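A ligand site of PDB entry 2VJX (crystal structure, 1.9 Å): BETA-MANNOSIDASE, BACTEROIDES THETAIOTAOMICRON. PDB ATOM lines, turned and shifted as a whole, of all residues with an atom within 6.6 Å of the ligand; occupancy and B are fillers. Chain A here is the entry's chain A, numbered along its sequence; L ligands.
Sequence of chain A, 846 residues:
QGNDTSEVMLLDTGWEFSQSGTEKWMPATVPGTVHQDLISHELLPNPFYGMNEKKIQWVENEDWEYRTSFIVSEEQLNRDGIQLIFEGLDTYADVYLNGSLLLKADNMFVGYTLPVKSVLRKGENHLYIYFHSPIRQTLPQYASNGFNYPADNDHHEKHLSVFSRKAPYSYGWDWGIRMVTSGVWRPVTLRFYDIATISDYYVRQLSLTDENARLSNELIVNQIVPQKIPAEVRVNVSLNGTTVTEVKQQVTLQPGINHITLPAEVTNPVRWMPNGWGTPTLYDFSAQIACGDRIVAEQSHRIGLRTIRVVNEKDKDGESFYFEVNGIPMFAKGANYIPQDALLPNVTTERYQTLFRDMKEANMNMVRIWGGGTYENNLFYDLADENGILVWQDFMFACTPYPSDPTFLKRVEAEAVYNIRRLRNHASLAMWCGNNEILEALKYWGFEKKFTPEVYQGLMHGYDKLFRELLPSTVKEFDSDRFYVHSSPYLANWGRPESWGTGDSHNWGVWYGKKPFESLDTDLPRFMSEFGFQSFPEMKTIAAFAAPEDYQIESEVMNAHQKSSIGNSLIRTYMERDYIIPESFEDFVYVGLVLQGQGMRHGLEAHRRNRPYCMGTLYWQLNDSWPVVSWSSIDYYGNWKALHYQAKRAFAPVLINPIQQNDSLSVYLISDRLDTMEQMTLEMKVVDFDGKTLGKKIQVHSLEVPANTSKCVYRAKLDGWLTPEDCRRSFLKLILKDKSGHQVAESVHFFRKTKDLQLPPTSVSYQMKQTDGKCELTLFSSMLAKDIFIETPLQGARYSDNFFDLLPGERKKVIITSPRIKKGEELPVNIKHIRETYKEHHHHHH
O3 of the ligand sits at hydrogen-bond distance from OH of Tyr 512 (2.6 Å).
OE1 of Glu 530 is in hydrogen-bond range of N1 of the ligand, at 2.8 Å.
An oxygen (O1) of the ligand lies within hydrogen-bond range of the side-chain carboxylate (OD1) of Asp 174 (2.6 Å).
The side-chain amide nitrogen of Asn 436 lies within hydrogen-bond range of an oxygen (O4) of the ligand (2.8 Å).
NE1 of Trp 173 lies within hydrogen-bond range of O2 of the ligand, 2.9 Å away.
An oxygen (O1) of the ligand lies within hydrogen-bond range of the indole nitrogen (NE1) of Trp 175 (3.0 Å).
An oxygen (O4) of the ligand is in hydrogen-bond range of the indole nitrogen of Trp 370 (3.0 Å).
OE2 of Glu 437 sits at hydrogen-bond distance from N1 of the ligand, 3.3 Å away.
SG of Cys 399 sits at hydrogen-bond distance from O2 of the ligand (3.7 Å).
OD1 of Asn 436 lies close to OE2 of Glu 530 (3.0 Å).
The indole nitrogen (NE1) of Trp 508 is in hydrogen-bond range of the side-chain carboxylate (OE1) of Glu 530 (3.0 Å).
A ring nitrogen (ND1) of His 506 is in hydrogen-bond range of the side-chain carboxylate of Glu 530 (3.1 Å).
The guanidinium group of Arg 368 lies within salt-bridge range of the side-chain carboxylate of Glu 530.
The side-chain amide nitrogen (ND2) of Asn 436 sits close to the indole nitrogen (NE1) of Trp 370 (3.3 Å).
The backbone NH (N) of Cys 399 sits at hydrogen-bond distance from the backbone carbonyl oxygen (O) of Asn 436, at 2.8 Å.
A ring nitrogen (ND1) of His 506 lies within hydrogen-bond range of the side-chain carboxylate (OE2) of Glu 437 (2.7 Å).
The indole nitrogen (NE1) of Trp 620 is in hydrogen-bond range of the side-chain amide oxygen (OE1) of Gln 621, 2.9 Å away.
Trp 508 touches the ligand.
Trp 620 touches the ligand.
CZ2 of Trp 631 touches C6 of the ligand, at 3.7 Å.
Hydrophobic or aromatic side chains within 4 Å of the ligand: Trp 173, Trp 175, Trp 370, Trp 508, Tyr 512, Trp 620 and Trp 631.
Within 4 Å of the ligand: Trp 173, Asp 174, Trp 175, Trp 370, Cys 399, Asn 436, Glu 437, Trp 508, Tyr 512, Glu 530, Trp 620 and Trp 631.
Along chain A the residues within 4 Å of the ligand span positions 173 to 631.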
ATOM      1  N   ASN A 153      33.672  -3.955  11.567  1.00  0.00           N
ATOM      2  CA  ASN A 153      32.627  -4.668  12.281  1.00  0.00           C
ATOM      3  C   ASN A 153      32.338  -6.064  11.749  1.00  0.00           C
ATOM      4  O   ASN A 153      31.619  -6.803  12.400  1.00  0.00           O
ATOM      5  CB  ASN A 153      31.345  -3.836  12.371  1.00  0.00           C
ATOM      6  CG  ASN A 153      31.469  -2.689  13.395  1.00  0.00           C
ATOM      7  OD1 ASN A 153      31.556  -2.934  14.615  1.00  0.00           O
ATOM      8  ND2 ASN A 153      31.443  -1.458  12.912  1.00  0.00           N
ATOM      9  N   TRP A 173      29.141  -7.248  15.145  1.00  0.00           N
ATOM     10  CA  TRP A 173      29.202  -5.790  15.290  1.00  0.00           C
ATOM     11  C   TRP A 173      29.819  -5.496  16.673  1.00  0.00           C
ATOM     12  O   TRP A 173      30.130  -6.445  17.420  1.00  0.00           O
ATOM     13  CB  TRP A 173      27.785  -5.162  15.182  1.00  0.00           C
ATOM     14  CG  TRP A 173      27.879  -3.770  14.583  1.00  0.00           C
ATOM     15  CD1 TRP A 173      27.902  -2.592  15.252  1.00  0.00           C
ATOM     16  CD2 TRP A 173      27.950  -3.441  13.184  1.00  0.00           C
ATOM     17  NE1 TRP A 173      28.015  -1.540  14.385  1.00  0.00           N
ATOM     18  CE2 TRP A 173      28.050  -2.030  13.098  1.00  0.00           C
ATOM     19  CE3 TRP A 173      27.940  -4.205  12.004  1.00  0.00           C
ATOM     20  CZ2 TRP A 173      28.177  -1.361  11.881  1.00  0.00           C
ATOM     21  CZ3 TRP A 173      28.065  -3.531  10.758  1.00  0.00           C
ATOM     22  CH2 TRP A 173      28.158  -2.107  10.715  1.00  0.00           C
ATOM     23  N   ASP A 174      29.959  -4.223  17.047  1.00  0.00           N
ATOM     24  CA  ASP A 174      30.633  -3.895  18.332  1.00  0.00           C
ATOM     25  C   ASP A 174      29.696  -4.035  19.561  1.00  0.00           C
ATOM     26  O   ASP A 174      30.093  -3.730  20.686  1.00  0.00           O
ATOM     27  CB  ASP A 174      31.389  -2.546  18.273  1.00  0.00           C
ATOM     28  CG  ASP A 174      30.465  -1.339  17.969  1.00  0.00           C
ATOM     29  OD1 ASP A 174      29.207  -1.457  18.065  1.00  0.00           O
ATOM     30  OD2 ASP A 174      31.044  -0.251  17.672  1.00  0.00           O
ATOM     31  N   TRP A 175      28.456  -4.499  19.323  1.00  0.00           N
ATOM     32  CA  TRP A 175      27.528  -5.006  20.365  1.00  0.00           C
ATOM     33  C   TRP A 175      26.908  -6.342  19.933  1.00  0.00           C
ATOM     34  O   TRP A 175      25.888  -6.763  20.503  1.00  0.00           O
ATOM     35  CB  TRP A 175      26.340  -4.020  20.597  1.00  0.00           C
ATOM     36  CG  TRP A 175      25.894  -3.365  19.299  1.00  0.00           C
ATOM     37  CD1 TRP A 175      26.167  -2.101  18.898  1.00  0.00           C
ATOM     38  CD2 TRP A 175      25.131  -3.981  18.224  1.00  0.00           C
ATOM     39  NE1 TRP A 175      25.623  -1.881  17.627  1.00  0.00           N
ATOM     40  CE2 TRP A 175      24.997  -3.014  17.202  1.00  0.00           C
ATOM     41  CE3 TRP A 175      24.576  -5.266  18.025  1.00  0.00           C
ATOM     42  CZ2 TRP A 175      24.298  -3.259  16.002  1.00  0.00           C
ATOM     43  CZ3 TRP A 175      23.890  -5.530  16.828  1.00  0.00           C
ATOM     44  CH2 TRP A 175      23.773  -4.536  15.837  1.00  0.00           C
ATOM     45  N   ASN A 336      17.948   5.132  18.448  1.00  0.00           N
ATOM     46  CA  ASN A 336      18.374   4.274  17.343  1.00  0.00           C
ATOM     47  C   ASN A 336      18.054   2.815  17.626  1.00  0.00           C
ATOM     48  O   ASN A 336      18.417   2.255  18.694  1.00  0.00           O
ATOM     49  CB  ASN A 336      19.881   4.430  17.115  1.00  0.00           C
ATOM     50  CG  ASN A 336      20.244   5.766  16.498  1.00  0.00           C
ATOM     51  OD1 ASN A 336      20.414   5.856  15.270  1.00  0.00           O
ATOM     52  ND2 ASN A 336      20.433   6.811  17.344  1.00  0.00           N
ATOM     53  N   ILE A 338      18.183  -1.195  16.553  1.00  0.00           N
ATOM     54  CA  ILE A 338      18.942  -2.268  15.903  1.00  0.00           C
ATOM     55  C   ILE A 338      18.068  -3.536  15.867  1.00  0.00           C
ATOM     56  O   ILE A 338      17.001  -3.581  16.485  1.00  0.00           O
ATOM     57  CB  ILE A 338      20.292  -2.539  16.643  1.00  0.00           C
ATOM     58  CG1 ILE A 338      20.026  -3.163  18.052  1.00  0.00           C
ATOM     59  CG2 ILE A 338      21.192  -1.287  16.678  1.00  0.00           C
ATOM     60  CD1 ILE A 338      21.217  -3.968  18.566  1.00  0.00           C
ATOM     61  N   ARG A 368      14.992   5.747  14.825  1.00  0.00           N
ATOM     62  CA  ARG A 368      15.831   5.579  13.646  1.00  0.00           C
ATOM     63  C   ARG A 368      16.146   4.092  13.401  1.00  0.00           C
ATOM     64  O   ARG A 368      16.708   3.420  14.309  1.00  0.00           O
ATOM     65  CB  ARG A 368      17.125   6.376  13.803  1.00  0.00           C
ATOM     66  CG  ARG A 368      18.107   6.118  12.610  1.00  0.00           C
ATOM     67  CD  ARG A 368      19.230   7.113  12.538  1.00  0.00           C
ATOM     68  NE  ARG A 368      20.225   6.691  11.569  1.00  0.00           N
ATOM     69  CZ  ARG A 368      21.532   6.550  11.836  1.00  0.00           C
ATOM     70  NH1 ARG A 368      22.020   6.812  13.074  1.00  0.00           N
ATOM     71  NH2 ARG A 368      22.361   6.156  10.857  1.00  0.00           N
ATOM     72  N   TRP A 370      18.436   1.933  12.058  1.00  0.00           N
ATOM     73  CA  TRP A 370      19.830   2.098  11.699  1.00  0.00           C
ATOM     74  C   TRP A 370      20.282   1.142  10.581  1.00  0.00           C
ATOM     75  O   TRP A 370      19.858  -0.031  10.515  1.00  0.00           O
ATOM     76  CB  TRP A 370      20.660   1.969  12.995  1.00  0.00           C
ATOM     77  CG  TRP A 370      22.111   1.720  12.872  1.00  0.00           C
ATOM     78  CD1 TRP A 370      23.114   2.662  12.868  1.00  0.00           C
ATOM     79  CD2 TRP A 370      22.743   0.439  12.890  1.00  0.00           C
ATOM     80  NE1 TRP A 370      24.340   2.037  12.823  1.00  0.00           N
ATOM     81  CE2 TRP A 370      24.143   0.667  12.858  1.00  0.00           C
ATOM     82  CE3 TRP A 370      22.272  -0.889  12.944  1.00  0.00           C
ATOM     83  CZ2 TRP A 370      25.068  -0.374  12.857  1.00  0.00           C
ATOM     84  CZ3 TRP A 370      23.210  -1.934  12.927  1.00  0.00           C
ATOM     85  CH2 TRP A 370      24.596  -1.658  12.881  1.00  0.00           C
ATOM     86  N   ALA A 398      26.323   0.525   6.256  1.00  0.00           N
ATOM     87  CA  ALA A 398      26.838   1.101   7.517  1.00  0.00           C
ATOM     88  C   ALA A 398      28.360   0.959   7.691  1.00  0.00           C
ATOM     89  O   ALA A 398      28.886  -0.150   7.593  1.00  0.00           O
ATOM     90  CB  ALA A 398      26.117   0.469   8.724  1.00  0.00           C
ATOM     91  N   CYS A 399      29.021   2.088   7.933  1.00  0.00           N
ATOM     92  CA  CYS A 399      30.406   2.177   8.491  1.00  0.00           C
ATOM     93  C   CYS A 399      31.569   1.693   7.596  1.00  0.00           C
ATOM     94  O   CYS A 399      32.690   1.534   8.104  1.00  0.00           O
ATOM     95  CB  CYS A 399      30.520   1.467   9.847  1.00  0.00           C
ATOM     96  SG  CYS A 399      29.337   2.015  11.087  1.00  0.00           S
ATOM     97  N   ASN A 436      24.680   4.829   7.307  1.00  0.00           N
ATOM     98  CA  ASN A 436      25.257   5.238   8.581  1.00  0.00           C
ATOM     99  C   ASN A 436      26.781   5.429   8.475  1.00  0.00           C
ATOM    100  O   ASN A 436      27.517   4.463   8.219  1.00  0.00           O
ATOM    101  CB  ASN A 436      24.950   4.176   9.667  1.00  0.00           C
ATOM    102  CG  ASN A 436      25.496   4.578  11.009  1.00  0.00           C
ATOM    103  OD1 ASN A 436      24.958   5.484  11.654  1.00  0.00           O
ATOM    104  ND2 ASN A 436      26.599   3.946  11.397  1.00  0.00           N
ATOM    105  N   GLU A 437      27.247   6.669   8.697  1.00  0.00           N
ATOM    106  CA  GLU A 437      28.681   6.977   8.943  1.00  0.00           C
ATOM    107  C   GLU A 437      29.656   6.731   7.793  1.00  0.00           C
ATOM    108  O   GLU A 437      30.871   6.808   8.007  1.00  0.00           O
ATOM    109  CB  GLU A 437      29.186   6.349  10.266  1.00  0.00           C
ATOM    110  CG  GLU A 437      28.534   7.020  11.491  1.00  0.00           C
ATOM    111  CD  GLU A 437      28.826   6.297  12.835  1.00  0.00           C
ATOM    112  OE1 GLU A 437      29.453   5.208  12.824  1.00  0.00           O
ATOM    113  OE2 GLU A 437      28.380   6.815  13.892  1.00  0.00           O
ATOM    114  N   HIS A 506      26.556  12.831  15.182  1.00  0.00           N
ATOM    115  CA  HIS A 506      26.795  11.671  16.074  1.00  0.00           C
ATOM    116  C   HIS A 506      27.903  12.102  17.022  1.00  0.00           C
ATOM    117  O   HIS A 506      29.094  11.956  16.711  1.00  0.00           O
ATOM    118  CB  HIS A 506      27.298  10.431  15.302  1.00  0.00           C
ATOM    119  CG  HIS A 506      26.327   9.906  14.282  1.00  0.00           C
ATOM    120  ND1 HIS A 506      26.461   8.658  13.721  1.00  0.00           N
ATOM    121  CD2 HIS A 506      25.208  10.443  13.755  1.00  0.00           C
ATOM    122  CE1 HIS A 506      25.476   8.456  12.860  1.00  0.00           C
ATOM    123  NE2 HIS A 506      24.680   9.509  12.880  1.00  0.00           N
ATOM    124  N   TRP A 508      30.180  11.464  19.428  1.00  0.00           N
ATOM    125  CA  TRP A 508      30.890  10.416  20.129  1.00  0.00           C
ATOM    126  C   TRP A 508      32.080  10.972  20.930  1.00  0.00           C
ATOM    127  O   TRP A 508      33.000  10.245  21.283  1.00  0.00           O
ATOM    128  CB  TRP A 508      31.300   9.271  19.172  1.00  0.00           C
ATOM    129  CG  TRP A 508      30.084   8.465  18.857  1.00  0.00           C
ATOM    130  CD1 TRP A 508      29.391   8.466  17.685  1.00  0.00           C
ATOM    131  CD2 TRP A 508      29.364   7.599  19.759  1.00  0.00           C
ATOM    132  NE1 TRP A 508      28.283   7.647  17.789  1.00  0.00           N
ATOM    133  CE2 TRP A 508      28.244   7.103  19.048  1.00  0.00           C
ATOM    134  CE3 TRP A 508      29.564   7.188  21.098  1.00  0.00           C
ATOM    135  CZ2 TRP A 508      27.327   6.181  19.615  1.00  0.00           C
ATOM    136  CZ3 TRP A 508      28.640   6.293  21.691  1.00  0.00           C
ATOM    137  CH2 TRP A 508      27.531   5.796  20.935  1.00  0.00           C
ATOM    138  N   TRP A 511      31.967   9.087  25.519  1.00  0.00           N
ATOM    139  CA  TRP A 511      32.351   7.684  25.208  1.00  0.00           C
ATOM    140  C   TRP A 511      33.699   7.653  24.455  1.00  0.00           C
ATOM    141  O   TRP A 511      34.767   7.663  25.103  1.00  0.00           O
ATOM    142  CB  TRP A 511      31.185   6.858  24.556  1.00  0.00           C
ATOM    143  CG  TRP A 511      31.581   5.380  24.451  1.00  0.00           C
ATOM    144  CD1 TRP A 511      32.045   4.739  23.330  1.00  0.00           C
ATOM    145  CD2 TRP A 511      31.624   4.407  25.521  1.00  0.00           C
ATOM    146  NE1 TRP A 511      32.336   3.426  23.642  1.00  0.00           N
ATOM    147  CE2 TRP A 511      32.090   3.198  24.974  1.00  0.00           C
ATOM    148  CE3 TRP A 511      31.316   4.448  26.900  1.00  0.00           C
ATOM    149  CZ2 TRP A 511      32.277   2.029  25.749  1.00  0.00           C
ATOM    150  CZ3 TRP A 511      31.475   3.303  27.670  1.00  0.00           C
ATOM    151  CH2 TRP A 511      31.958   2.099  27.082  1.00  0.00           C
ATOM    152  N   TYR A 512      33.699   7.668  23.117  1.00  0.00           N
ATOM    153  CA  TYR A 512      34.946   7.517  22.337  1.00  0.00           C
ATOM    154  C   TYR A 512      35.960   8.629  22.628  1.00  0.00           C
ATOM    155  O   TYR A 512      37.163   8.350  22.727  1.00  0.00           O
ATOM    156  CB  TYR A 512      34.705   7.407  20.836  1.00  0.00           C
ATOM    157  CG  TYR A 512      34.075   6.055  20.520  1.00  0.00           C
ATOM    158  CD1 TYR A 512      34.731   4.871  20.907  1.00  0.00           C
ATOM    159  CD2 TYR A 512      32.813   5.947  19.936  1.00  0.00           C
ATOM    160  CE1 TYR A 512      34.179   3.605  20.678  1.00  0.00           C
ATOM    161  CE2 TYR A 512      32.234   4.643  19.684  1.00  0.00           C
ATOM    162  CZ  TYR A 512      32.939   3.495  20.058  1.00  0.00           C
ATOM    163  OH  TYR A 512      32.434   2.227  19.894  1.00  0.00           O
ATOM    164  N   GLU A 530      22.895  10.574  16.981  1.00  0.00           N
ATOM    165  CA  GLU A 530      23.452   9.546  17.884  1.00  0.00           C
ATOM    166  C   GLU A 530      24.292  10.185  18.987  1.00  0.00           C
ATOM    167  O   GLU A 530      25.068  11.108  18.703  1.00  0.00           O
ATOM    168  CB  GLU A 530      24.449   8.620  17.124  1.00  0.00           C
ATOM    169  CG  GLU A 530      23.856   7.654  16.063  1.00  0.00           C
ATOM    170  CD  GLU A 530      24.898   6.640  15.565  1.00  0.00           C
ATOM    171  OE1 GLU A 530      26.034   6.633  16.087  1.00  0.00           O
ATOM    172  OE2 GLU A 530      24.563   5.828  14.644  1.00  0.00           O
ATOM    173  N   TRP A 620      21.945   6.485  21.070  1.00  0.00           N
ATOM    174  CA  TRP A 620      22.496   5.202  20.667  1.00  0.00           C
ATOM    175  C   TRP A 620      22.602   4.417  21.989  1.00  0.00           C
ATOM    176  O   TRP A 620      23.416   4.827  22.830  1.00  0.00           O
ATOM    177  CB  TRP A 620      23.920   5.380  20.037  1.00  0.00           C
ATOM    178  CG  TRP A 620      24.320   4.032  19.549  1.00  0.00           C
ATOM    179  CD1 TRP A 620      25.003   3.037  20.251  1.00  0.00           C
ATOM    180  CD2 TRP A 620      23.869   3.425  18.337  1.00  0.00           C
ATOM    181  NE1 TRP A 620      25.043   1.876  19.494  1.00  0.00           N
ATOM    182  CE2 TRP A 620      24.361   2.088  18.314  1.00  0.00           C
ATOM    183  CE3 TRP A 620      23.136   3.911  17.223  1.00  0.00           C
ATOM    184  CZ2 TRP A 620      24.079   1.210  17.260  1.00  0.00           C
ATOM    185  CZ3 TRP A 620      22.891   3.042  16.142  1.00  0.00           C
ATOM    186  CH2 TRP A 620      23.375   1.697  16.168  1.00  0.00           C
ATOM    187  N   GLN A 621      21.855   3.332  22.218  1.00  0.00           N
ATOM    188  CA  GLN A 621      20.941   2.698  21.266  1.00  0.00           C
ATOM    189  C   GLN A 621      19.683   2.269  22.085  1.00  0.00           C
ATOM    190  O   GLN A 621      19.746   2.152  23.323  1.00  0.00           O
ATOM    191  CB  GLN A 621      21.621   1.453  20.650  1.00  0.00           C
ATOM    192  CG  GLN A 621      21.858   0.247  21.609  1.00  0.00           C
ATOM    193  CD  GLN A 621      23.015  -0.664  21.182  1.00  0.00           C
ATOM    194  OE1 GLN A 621      24.198  -0.288  21.297  1.00  0.00           O
ATOM    195  NE2 GLN A 621      22.689  -1.865  20.701  1.00  0.00           N
ATOM    196  N   TRP A 631      25.355  -0.191  24.574  1.00  0.00           N
ATOM    197  CA  TRP A 631      24.805   1.150  24.773  1.00  0.00           C
ATOM    198  C   TRP A 631      23.276   1.159  24.941  1.00  0.00           C
ATOM    199  O   TRP A 631      22.662   2.214  25.027  1.00  0.00           O
ATOM    200  CB  TRP A 631      25.191   2.014  23.565  1.00  0.00           C
ATOM    201  CG  TRP A 631      26.698   2.119  23.356  1.00  0.00           C
ATOM    202  CD1 TRP A 631      27.500   3.165  23.751  1.00  0.00           C
ATOM    203  CD2 TRP A 631      27.584   1.164  22.714  1.00  0.00           C
ATOM    204  NE1 TRP A 631      28.808   2.911  23.397  1.00  0.00           N
ATOM    205  CE2 TRP A 631      28.884   1.692  22.780  1.00  0.00           C
ATOM    206  CE3 TRP A 631      27.373  -0.088  22.065  1.00  0.00           C
ATOM    207  CZ2 TRP A 631      30.019   1.022  22.216  1.00  0.00           C
ATOM    208  CZ3 TRP A 631      28.479  -0.769  21.521  1.00  0.00           C
ATOM    209  CH2 TRP A 631      29.799  -0.209  21.605  1.00  0.00           C
HETATM  210  O1  LIG L   1      27.540   0.322  17.098  1.00  0.00           O
HETATM  211  C1  LIG L   1      28.014   1.572  16.571  1.00  0.00           C
HETATM  212  C2  LIG L   1      27.071   1.970  15.412  1.00  0.00           C
HETATM  213  O2  LIG L   1      27.587   1.361  14.230  1.00  0.00           O
HETATM  214  C3  LIG L   1      26.964   3.496  15.124  1.00  0.00           C
HETATM  215  N1  LIG L   1      27.671   4.337  15.921  1.00  0.00           N
HETATM  216  C4  LIG L   1      28.467   3.978  17.095  1.00  0.00           C
HETATM  217  C5  LIG L   1      27.993   2.630  17.682  1.00  0.00           C
HETATM  218  C6  LIG L   1      28.788   2.174  18.940  1.00  0.00           C
HETATM  219  O3  LIG L   1      30.186   2.136  18.652  1.00  0.00           O
HETATM  220  O4  LIG L   1      26.287   3.942  14.186  1.00  0.00           O
